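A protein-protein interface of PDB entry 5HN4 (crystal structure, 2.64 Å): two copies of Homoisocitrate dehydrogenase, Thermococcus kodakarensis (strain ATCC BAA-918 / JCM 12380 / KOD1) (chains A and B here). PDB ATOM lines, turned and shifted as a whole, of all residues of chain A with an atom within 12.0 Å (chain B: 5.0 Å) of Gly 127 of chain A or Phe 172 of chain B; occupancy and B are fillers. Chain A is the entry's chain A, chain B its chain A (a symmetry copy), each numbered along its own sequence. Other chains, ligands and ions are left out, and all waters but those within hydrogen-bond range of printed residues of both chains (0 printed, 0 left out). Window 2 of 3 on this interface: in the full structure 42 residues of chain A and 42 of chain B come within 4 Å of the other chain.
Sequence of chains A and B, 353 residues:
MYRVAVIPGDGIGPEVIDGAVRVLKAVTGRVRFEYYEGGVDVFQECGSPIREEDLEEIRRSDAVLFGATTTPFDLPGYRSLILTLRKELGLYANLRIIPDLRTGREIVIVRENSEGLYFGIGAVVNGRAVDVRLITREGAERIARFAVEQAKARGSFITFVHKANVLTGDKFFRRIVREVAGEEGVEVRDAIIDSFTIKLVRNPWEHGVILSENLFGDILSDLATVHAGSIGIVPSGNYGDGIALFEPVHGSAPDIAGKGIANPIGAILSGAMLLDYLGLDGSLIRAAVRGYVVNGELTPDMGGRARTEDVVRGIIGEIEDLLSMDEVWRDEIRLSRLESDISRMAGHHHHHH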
ATOM      1  N   PHE A  73     -16.658  -1.819   4.520  1.00  0.00           N
ATOM      2  CA  PHE A  73     -16.139  -0.715   3.700  1.00  0.00           C
ATOM      3  C   PHE A  73     -17.005   0.552   3.827  1.00  0.00           C
ATOM      4  O   PHE A  73     -16.502   1.660   3.654  1.00  0.00           O
ATOM      5  CB  PHE A  73     -15.988  -1.139   2.216  1.00  0.00           C
ATOM      6  CG  PHE A  73     -17.302  -1.334   1.486  1.00  0.00           C
ATOM      7  CD1 PHE A  73     -18.031  -2.525   1.610  1.00  0.00           C
ATOM      8  CD2 PHE A  73     -17.809  -0.331   0.652  1.00  0.00           C
ATOM      9  CE1 PHE A  73     -19.232  -2.701   0.929  1.00  0.00           C
ATOM     10  CE2 PHE A  73     -19.016  -0.506  -0.028  1.00  0.00           C
ATOM     11  CZ  PHE A  73     -19.725  -1.691   0.110  1.00  0.00           C
ATOM     12  N   GLY A 122      -1.870   9.484   3.539  1.00  0.00           N
ATOM     13  CA  GLY A 122      -2.643   9.515   2.301  1.00  0.00           C
ATOM     14  C   GLY A 122      -3.572  10.716   2.235  1.00  0.00           C
ATOM     15  O   GLY A 122      -4.065  11.174   3.243  1.00  0.00           O
ATOM     16  N   ALA A 123      -3.860  11.169   1.026  1.00  0.00           N
ATOM     17  CA  ALA A 123      -4.539  12.422   0.791  1.00  0.00           C
ATOM     18  C   ALA A 123      -5.211  12.445  -0.580  1.00  0.00           C
ATOM     19  O   ALA A 123      -4.677  11.867  -1.529  1.00  0.00           O
ATOM     20  CB  ALA A 123      -3.511  13.531   0.861  1.00  0.00           C
ATOM     21  N   VAL A 124      -6.369  13.104  -0.672  1.00  0.00           N
ATOM     22  CA  VAL A 124      -6.982  13.483  -1.942  1.00  0.00           C
ATOM     23  C   VAL A 124      -7.019  15.000  -2.029  1.00  0.00           C
ATOM     24  O   VAL A 124      -7.507  15.643  -1.135  1.00  0.00           O
ATOM     25  CB  VAL A 124      -8.434  13.031  -2.073  1.00  0.00           C
ATOM     26  CG1 VAL A 124      -8.890  13.176  -3.522  1.00  0.00           C
ATOM     27  CG2 VAL A 124      -8.600  11.599  -1.675  1.00  0.00           C
ATOM     28  N   VAL A 125      -6.522  15.572  -3.109  1.00  0.00           N
ATOM     29  CA  VAL A 125      -6.547  17.014  -3.277  1.00  0.00           C
ATOM     30  C   VAL A 125      -6.440  17.393  -4.748  1.00  0.00           C
ATOM     31  O   VAL A 125      -5.391  17.161  -5.369  1.00  0.00           O
ATOM     32  CB  VAL A 125      -5.403  17.683  -2.491  1.00  0.00           C
ATOM     33  CG1 VAL A 125      -4.031  17.124  -2.906  1.00  0.00           C
ATOM     34  CG2 VAL A 125      -5.475  19.203  -2.646  1.00  0.00           C
ATOM     35  N   ASN A 126      -7.532  17.954  -5.283  1.00  0.00           N
ATOM     36  CA  ASN A 126      -7.606  18.494  -6.653  1.00  0.00           C
ATOM     37  C   ASN A 126      -7.592  17.391  -7.706  1.00  0.00           C
ATOM     38  O   ASN A 126      -6.793  17.447  -8.653  1.00  0.00           O
ATOM     39  CB  ASN A 126      -6.464  19.509  -6.980  1.00  0.00           C
ATOM     40  CG  ASN A 126      -6.365  20.670  -5.989  1.00  0.00           C
ATOM     41  OD1 ASN A 126      -5.282  21.233  -5.790  1.00  0.00           O
ATOM     42  ND2 ASN A 126      -7.488  21.042  -5.375  1.00  0.00           N
ATOM     43  N   GLY A 127      -8.467  16.398  -7.546  1.00  0.00           N
ATOM     44  CA  GLY A 127      -8.459  15.218  -8.417  1.00  0.00           C
ATOM     45  C   GLY A 127      -7.122  14.452  -8.494  1.00  0.00           C
ATOM     46  O   GLY A 127      -6.801  13.867  -9.519  1.00  0.00           O
ATOM     47  N   ARG A 128      -6.339  14.458  -7.419  1.00  0.00           N
ATOM     48  CA  ARG A 128      -5.153  13.647  -7.348  1.00  0.00           C
ATOM     49  C   ARG A 128      -5.157  12.970  -5.986  1.00  0.00           C
ATOM     50  O   ARG A 128      -5.177  13.639  -4.961  1.00  0.00           O
ATOM     51  CB  ARG A 128      -3.895  14.501  -7.509  1.00  0.00           C
ATOM     52  CG  ARG A 128      -3.977  15.511  -8.642  1.00  0.00           C
ATOM     53  CD  ARG A 128      -2.721  16.364  -8.754  1.00  0.00           C
ATOM     54  NE  ARG A 128      -1.837  15.904  -9.833  1.00  0.00           N
ATOM     55  CZ  ARG A 128      -0.589  15.448  -9.686  1.00  0.00           C
ATOM     56  NH1 ARG A 128      -0.011  15.369  -8.485  1.00  0.00           N
ATOM     57  NH2 ARG A 128       0.094  15.064 -10.765  1.00  0.00           N
ATOM     58  N   ALA A 129      -5.148  11.646  -5.970  1.00  0.00           N
ATOM     59  CA  ALA A 129      -5.087  10.891  -4.719  1.00  0.00           C
ATOM     60  C   ALA A 129      -3.725  10.255  -4.554  1.00  0.00           C
ATOM     61  O   ALA A 129      -3.114   9.812  -5.506  1.00  0.00           O
ATOM     62  CB  ALA A 129      -6.159   9.829  -4.701  1.00  0.00           C
ATOM     63  N   VAL A 130      -3.264  10.152  -3.328  1.00  0.00           N
ATOM     64  CA  VAL A 130      -1.909   9.751  -3.110  1.00  0.00           C
ATOM     65  C   VAL A 130      -1.819   8.834  -1.896  1.00  0.00           C
ATOM     66  O   VAL A 130      -2.660   8.922  -1.035  1.00  0.00           O
ATOM     67  CB  VAL A 130      -1.107  11.044  -3.018  1.00  0.00           C
ATOM     68  CG1 VAL A 130      -0.114  11.039  -1.902  1.00  0.00           C
ATOM     69  CG2 VAL A 130      -0.453  11.309  -4.355  1.00  0.00           C
ATOM     70  N   ASP A 131      -0.859   7.893  -1.877  1.00  0.00           N
ATOM     71  CA  ASP A 131      -0.522   7.103  -0.682  1.00  0.00           C
ATOM     72  C   ASP A 131       0.975   6.971  -0.713  1.00  0.00           C
ATOM     73  O   ASP A 131       1.539   6.760  -1.783  1.00  0.00           O
ATOM     74  CB  ASP A 131      -1.146   5.709  -0.679  1.00  0.00           C
ATOM     75  CG  ASP A 131      -2.658   5.709  -0.377  1.00  0.00           C
ATOM     76  OD1 ASP A 131      -3.047   5.695   0.807  1.00  0.00           O
ATOM     77  OD2 ASP A 131      -3.470   5.684  -1.308  1.00  0.00           O
ATOM     78  N   ILE B 135      -2.882   8.233  -7.893  1.00  0.00           N
ATOM     79  CA  ILE B 135      -4.021   8.019  -8.765  1.00  0.00           C
ATOM     80  C   ILE B 135      -4.595   9.383  -9.108  1.00  0.00           C
ATOM     81  O   ILE B 135      -4.827  10.163  -8.207  1.00  0.00           O
ATOM     82  CB  ILE B 135      -5.107   7.249  -8.029  1.00  0.00           C
ATOM     83  CG1 ILE B 135      -4.530   6.004  -7.361  1.00  0.00           C
ATOM     84  CG2 ILE B 135      -6.242   6.901  -8.968  1.00  0.00           C
ATOM     85  CD1 ILE B 135      -3.908   4.998  -8.303  1.00  0.00           C
ATOM     86  N   THR B 136      -4.828   9.676 -10.386  1.00  0.00           N
ATOM     87  CA  THR B 136      -5.420  10.960 -10.802  1.00  0.00           C
ATOM     88  C   THR B 136      -6.797  10.708 -11.362  1.00  0.00           C
ATOM     89  O   THR B 136      -7.108   9.586 -11.756  1.00  0.00           O
ATOM     90  CB  THR B 136      -4.571  11.649 -11.867  1.00  0.00           C
ATOM     91  OG1 THR B 136      -4.488  10.825 -13.051  1.00  0.00           O
ATOM     92  CG2 THR B 136      -3.191  11.906 -11.350  1.00  0.00           C
ATOM     93  N   ARG B 137      -7.634  11.741 -11.380  1.00  0.00           N
ATOM     94  CA  ARG B 137      -8.977  11.653 -11.992  1.00  0.00           C
ATOM     95  C   ARG B 137      -8.840  11.282 -13.476  1.00  0.00           C
ATOM     96  O   ARG B 137      -9.519  10.386 -13.943  1.00  0.00           O
ATOM     97  CB  ARG B 137      -9.740  12.980 -11.829  1.00  0.00           C
ATOM     98  CG  ARG B 137     -11.125  13.018 -12.489  1.00  0.00           C
ATOM     99  CD  ARG B 137     -12.050  14.101 -11.931  1.00  0.00           C
ATOM    100  NE  ARG B 137     -12.495  13.807 -10.558  1.00  0.00           N
ATOM    101  CZ  ARG B 137     -13.400  12.873 -10.224  1.00  0.00           C
ATOM    102  NH1 ARG B 137     -13.727  12.693  -8.945  1.00  0.00           N
ATOM    103  NH2 ARG B 137     -13.984  12.104 -11.153  1.00  0.00           N
ATOM    104  N   THR B 168      -5.967   5.405   0.269  1.00  0.00           N
ATOM    105  CA  THR B 168      -6.832   6.513  -0.100  1.00  0.00           C
ATOM    106  C   THR B 168      -7.051   6.500  -1.599  1.00  0.00           C
ATOM    107  O   THR B 168      -8.159   6.705  -2.105  1.00  0.00           O
ATOM    108  CB  THR B 168      -6.151   7.814   0.267  1.00  0.00           C
ATOM    109  OG1 THR B 168      -5.804   7.791   1.658  1.00  0.00           O
ATOM    110  CG2 THR B 168      -7.034   8.971  -0.053  1.00  0.00           C
ATOM    111  N   GLY B 169      -5.975   6.264  -2.327  1.00  0.00           N
ATOM    112  CA  GLY B 169      -6.034   6.329  -3.769  1.00  0.00           C
ATOM    113  C   GLY B 169      -6.935   5.270  -4.377  1.00  0.00           C
ATOM    114  O   GLY B 169      -7.523   5.477  -5.425  1.00  0.00           O
ATOM    115  N   ASP B 170      -7.052   4.127  -3.731  1.00  0.00           N
ATOM    116  CA  ASP B 170      -7.987   3.138  -4.220  1.00  0.00           C
ATOM    117  C   ASP B 170      -9.423   3.487  -3.882  1.00  0.00           C
ATOM    118  O   ASP B 170     -10.319   3.091  -4.628  1.00  0.00           O
ATOM    119  CB  ASP B 170      -7.656   1.736  -3.668  1.00  0.00           C
ATOM    120  CG  ASP B 170      -6.673   0.976  -4.551  1.00  0.00           C
ATOM    121  OD1 ASP B 170      -6.379   1.460  -5.698  1.00  0.00           O
ATOM    122  OD2 ASP B 170      -6.213  -0.112  -4.091  1.00  0.00           O
ATOM    123  N   LYS B 171      -9.667   4.189  -2.766  1.00  0.00           N
ATOM    124  CA  LYS B 171     -11.054   4.639  -2.451  1.00  0.00           C
ATOM    125  C   LYS B 171     -11.501   5.560  -3.587  1.00  0.00           C
ATOM    126  O   LYS B 171     -12.532   5.363  -4.186  1.00  0.00           O
ATOM    127  CB  LYS B 171     -11.183   5.279  -1.039  1.00  0.00           C
ATOM    128  CG  LYS B 171     -10.954   4.281   0.112  1.00  0.00           C
ATOM    129  CD  LYS B 171     -11.585   4.606   1.478  1.00  0.00           C
ATOM    130  CE  LYS B 171     -10.646   5.388   2.408  1.00  0.00           C
ATOM    131  NZ  LYS B 171      -9.572   4.655   3.148  1.00  0.00           N
ATOM    132  N   PHE B 172     -10.637   6.487  -3.949  1.00  0.00           N
ATOM    133  CA  PHE B 172     -10.839   7.387  -5.081  1.00  0.00           C
ATOM    134  C   PHE B 172     -11.075   6.655  -6.402  1.00  0.00           C
ATOM    135  O   PHE B 172     -12.038   6.921  -7.137  1.00  0.00           O
ATOM    136  CB  PHE B 172      -9.564   8.220  -5.181  1.00  0.00           C
ATOM    137  CG  PHE B 172      -9.648   9.372  -6.104  1.00  0.00           C
ATOM    138  CD1 PHE B 172     -10.544  10.403  -5.865  1.00  0.00           C
ATOM    139  CD2 PHE B 172      -8.770   9.481  -7.168  1.00  0.00           C
ATOM    140  CE1 PHE B 172     -10.597  11.500  -6.715  1.00  0.00           C
ATOM    141  CE2 PHE B 172      -8.812  10.574  -8.009  1.00  0.00           C
ATOM    142  CZ  PHE B 172      -9.722  11.587  -7.787  1.00  0.00           C
ATOM    143  N   PHE B 173     -10.160   5.740  -6.696  1.00  0.00           N
ATOM    144  CA  PHE B 173     -10.141   5.006  -7.938  1.00  0.00           C
ATOM    145  C   PHE B 173     -11.448   4.214  -8.042  1.00  0.00           C
ATOM    146  O   PHE B 173     -12.080   4.209  -9.081  1.00  0.00           O
ATOM    147  CB  PHE B 173      -8.926   4.074  -7.893  1.00  0.00           C
ATOM    148  CG  PHE B 173      -8.499   3.487  -9.208  1.00  0.00           C
ATOM    149  CD1 PHE B 173      -9.208   3.671 -10.372  1.00  0.00           C
ATOM    150  CD2 PHE B 173      -7.345   2.721  -9.247  1.00  0.00           C
ATOM    151  CE1 PHE B 173      -8.764   3.117 -11.543  1.00  0.00           C
ATOM    152  CE2 PHE B 173      -6.888   2.154 -10.422  1.00  0.00           C
ATOM    153  CZ  PHE B 173      -7.603   2.342 -11.558  1.00  0.00           C
ATOM    154  N   ARG B 174     -11.858   3.569  -6.952  1.00  0.00           N
ATOM    155  CA  ARG B 174     -13.061   2.745  -6.945  1.00  0.00           C
ATOM    156  C   ARG B 174     -14.309   3.596  -7.262  1.00  0.00           C
ATOM    157  O   ARG B 174     -15.157   3.189  -8.055  1.00  0.00           O
ATOM    158  CB  ARG B 174     -13.209   2.064  -5.589  1.00  0.00           C
ATOM    159  CG  ARG B 174     -14.413   1.152  -5.414  1.00  0.00           C
ATOM    160  CD  ARG B 174     -14.466   0.662  -3.965  1.00  0.00           C
ATOM    161  NE  ARG B 174     -15.571  -0.267  -3.751  1.00  0.00           N
ATOM    162  CZ  ARG B 174     -16.874   0.071  -3.716  1.00  0.00           C
ATOM    163  NH1 ARG B 174     -17.805  -0.864  -3.547  1.00  0.00           N
ATOM    164  NH2 ARG B 174     -17.274   1.332  -3.876  1.00  0.00           N
ATOM    165  N   ARG B 175     -14.404   4.772  -6.632  1.00  0.00           N
ATOM    166  CA  ARG B 175     -15.538   5.627  -6.890  1.00  0.00           C
ATOM    167  C   ARG B 175     -15.585   6.010  -8.366  1.00  0.00           C
ATOM    168  O   ARG B 175     -16.657   5.905  -8.969  1.00  0.00           O
ATOM    169  CB  ARG B 175     -15.587   6.848  -5.963  1.00  0.00           C
ATOM    170  CG  ARG B 175     -16.575   6.695  -4.797  1.00  0.00           C
ATOM    171  CD  ARG B 175     -15.889   6.739  -3.435  1.00  0.00           C
ATOM    172  NE  ARG B 175     -14.800   7.717  -3.425  1.00  0.00           N
ATOM    173  CZ  ARG B 175     -14.009   7.895  -2.392  1.00  0.00           C
ATOM    174  NH1 ARG B 175     -14.240   7.160  -1.316  1.00  0.00           N
ATOM    175  NH2 ARG B 175     -13.013   8.790  -2.437  1.00  0.00           N
ATOM    176  N   ILE B 176     -14.455   6.389  -8.957  1.00  0.00           N
ATOM    177  CA  ILE B 176     -14.462   6.761 -10.366  1.00  0.00           C
ATOM    178  C   ILE B 176     -14.762   5.574 -11.262  1.00  0.00           C
ATOM    179  O   ILE B 176     -15.534   5.684 -12.195  1.00  0.00           O
ATOM    180  CB  ILE B 176     -13.151   7.407 -10.799  1.00  0.00           C
ATOM    181  CG1 ILE B 176     -13.033   8.782 -10.165  1.00  0.00           C
ATOM    182  CG2 ILE B 176     -13.094   7.521 -12.314  1.00  0.00           C
ATOM    183  CD1 ILE B 176     -11.666   9.405 -10.306  1.00  0.00           C
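O of Ala 123 of chain A is in hydrogen-bond range of N of Val 130 of chain A (2.9 Å).
Printed residues of chain B within 4 Å of Gly 122 of chain A: Thr 168.
Of the printed residues of chain B, Ala 123 of chain A touches Thr 168.
Val 125 of chain A touches none of the printed residues of chain B.
Asn 126 of chain A touches none of the printed residues of chain B.
Printed residues of chain B within 4 Å of Gly 127 of chain A: Thr 136 (3.5 Å), Arg 137 (2.9 Å) and Phe 172 (3.9 Å).
Of the printed residues of chain B, Ala 129 of chain A touches Ile 135, Gly 169 and Phe 172.
Ile 135 of chain B touches just these residues of chain A: Arg 128 and Ala 129.
Gly 169 of chain B touches just these residues of chain A: Ala 129 and Asp 131.
No residue of chain A comes within 4 Å of Asp 170 of chain B.
Of the printed residues of chain A, Phe 172 of chain B touches Val 124, Gly 127 and Ala 129.
No residue of chain A comes within 4 Å of Phe 173 of chain B.
Printed residues of chain A within 4 Å of Arg 174 of chain B: Phe 73 (3.7 Å).
No residue of chain A comes within 4 Å of Ile 176 of chain B.
The nearest printed residue of chain A that does not touch Phe 172 of chain B is Arg 128 of chain A (4.5 Å).
Of the 12 printed residues of chain B, 7 touch a printed residue of chain A.
Hydrophobic or aromatic side chains of chain A within 4 Å of the printed part of chain B: Phe 73, Val 124 and Ala 129.
Along chain A the printed residues that touch a printed residue of chain B span positions 73 to 131.
No position is printed for both chains.
N of Arg 137 of chain B is in hydrogen-bond range of O of Gly 127 of chain A, 2.9 Å away.
The backbone NH of Ala 129 of chain A is in hydrogen-bond range of the backbone carbonyl oxygen of Ile 135 of chain B (2.7 Å).
The side-chain carboxylate (OD2) of Asp 131 of chain A sits at hydrogen-bond distance from the backbone NH (N) of Thr 168 of chain B (3.0 Å).
N of Gly 169 of chain B is in hydrogen-bond range of OD2 of Asp 131 of chain A (2.8 Å).
Arg 174 of chain B touches Phe 73 of chain A.
OG1 of Thr 168 of chain B touches CA of Gly 122 of chain A, 3.7 Å away.
Thr 168 of chain B touches Ala 123 of chain A (OG1 to N, 3.9 Å).
Val 124 of chain A touches Phe 172 of chain B.
Gly 127 of chain A touches Thr 136 of chain B (O to CA, 3.5 Å).
CZ of Phe 172 of chain B touches CA of Gly 127 of chain A, 3.9 Å away.
Arg 128 of chain A touches Ile 135 of chain B.
CB of Ala 129 of chain A touches CA of Gly 169 of chain B, 3.6 Å away.
CB of Ala 129 of chain A touches CD2 of Phe 172 of chain B, at 3.6 Å.
O of Val 130 of chain A touches CB of Thr 168 of chain B, 3.9 Å away.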
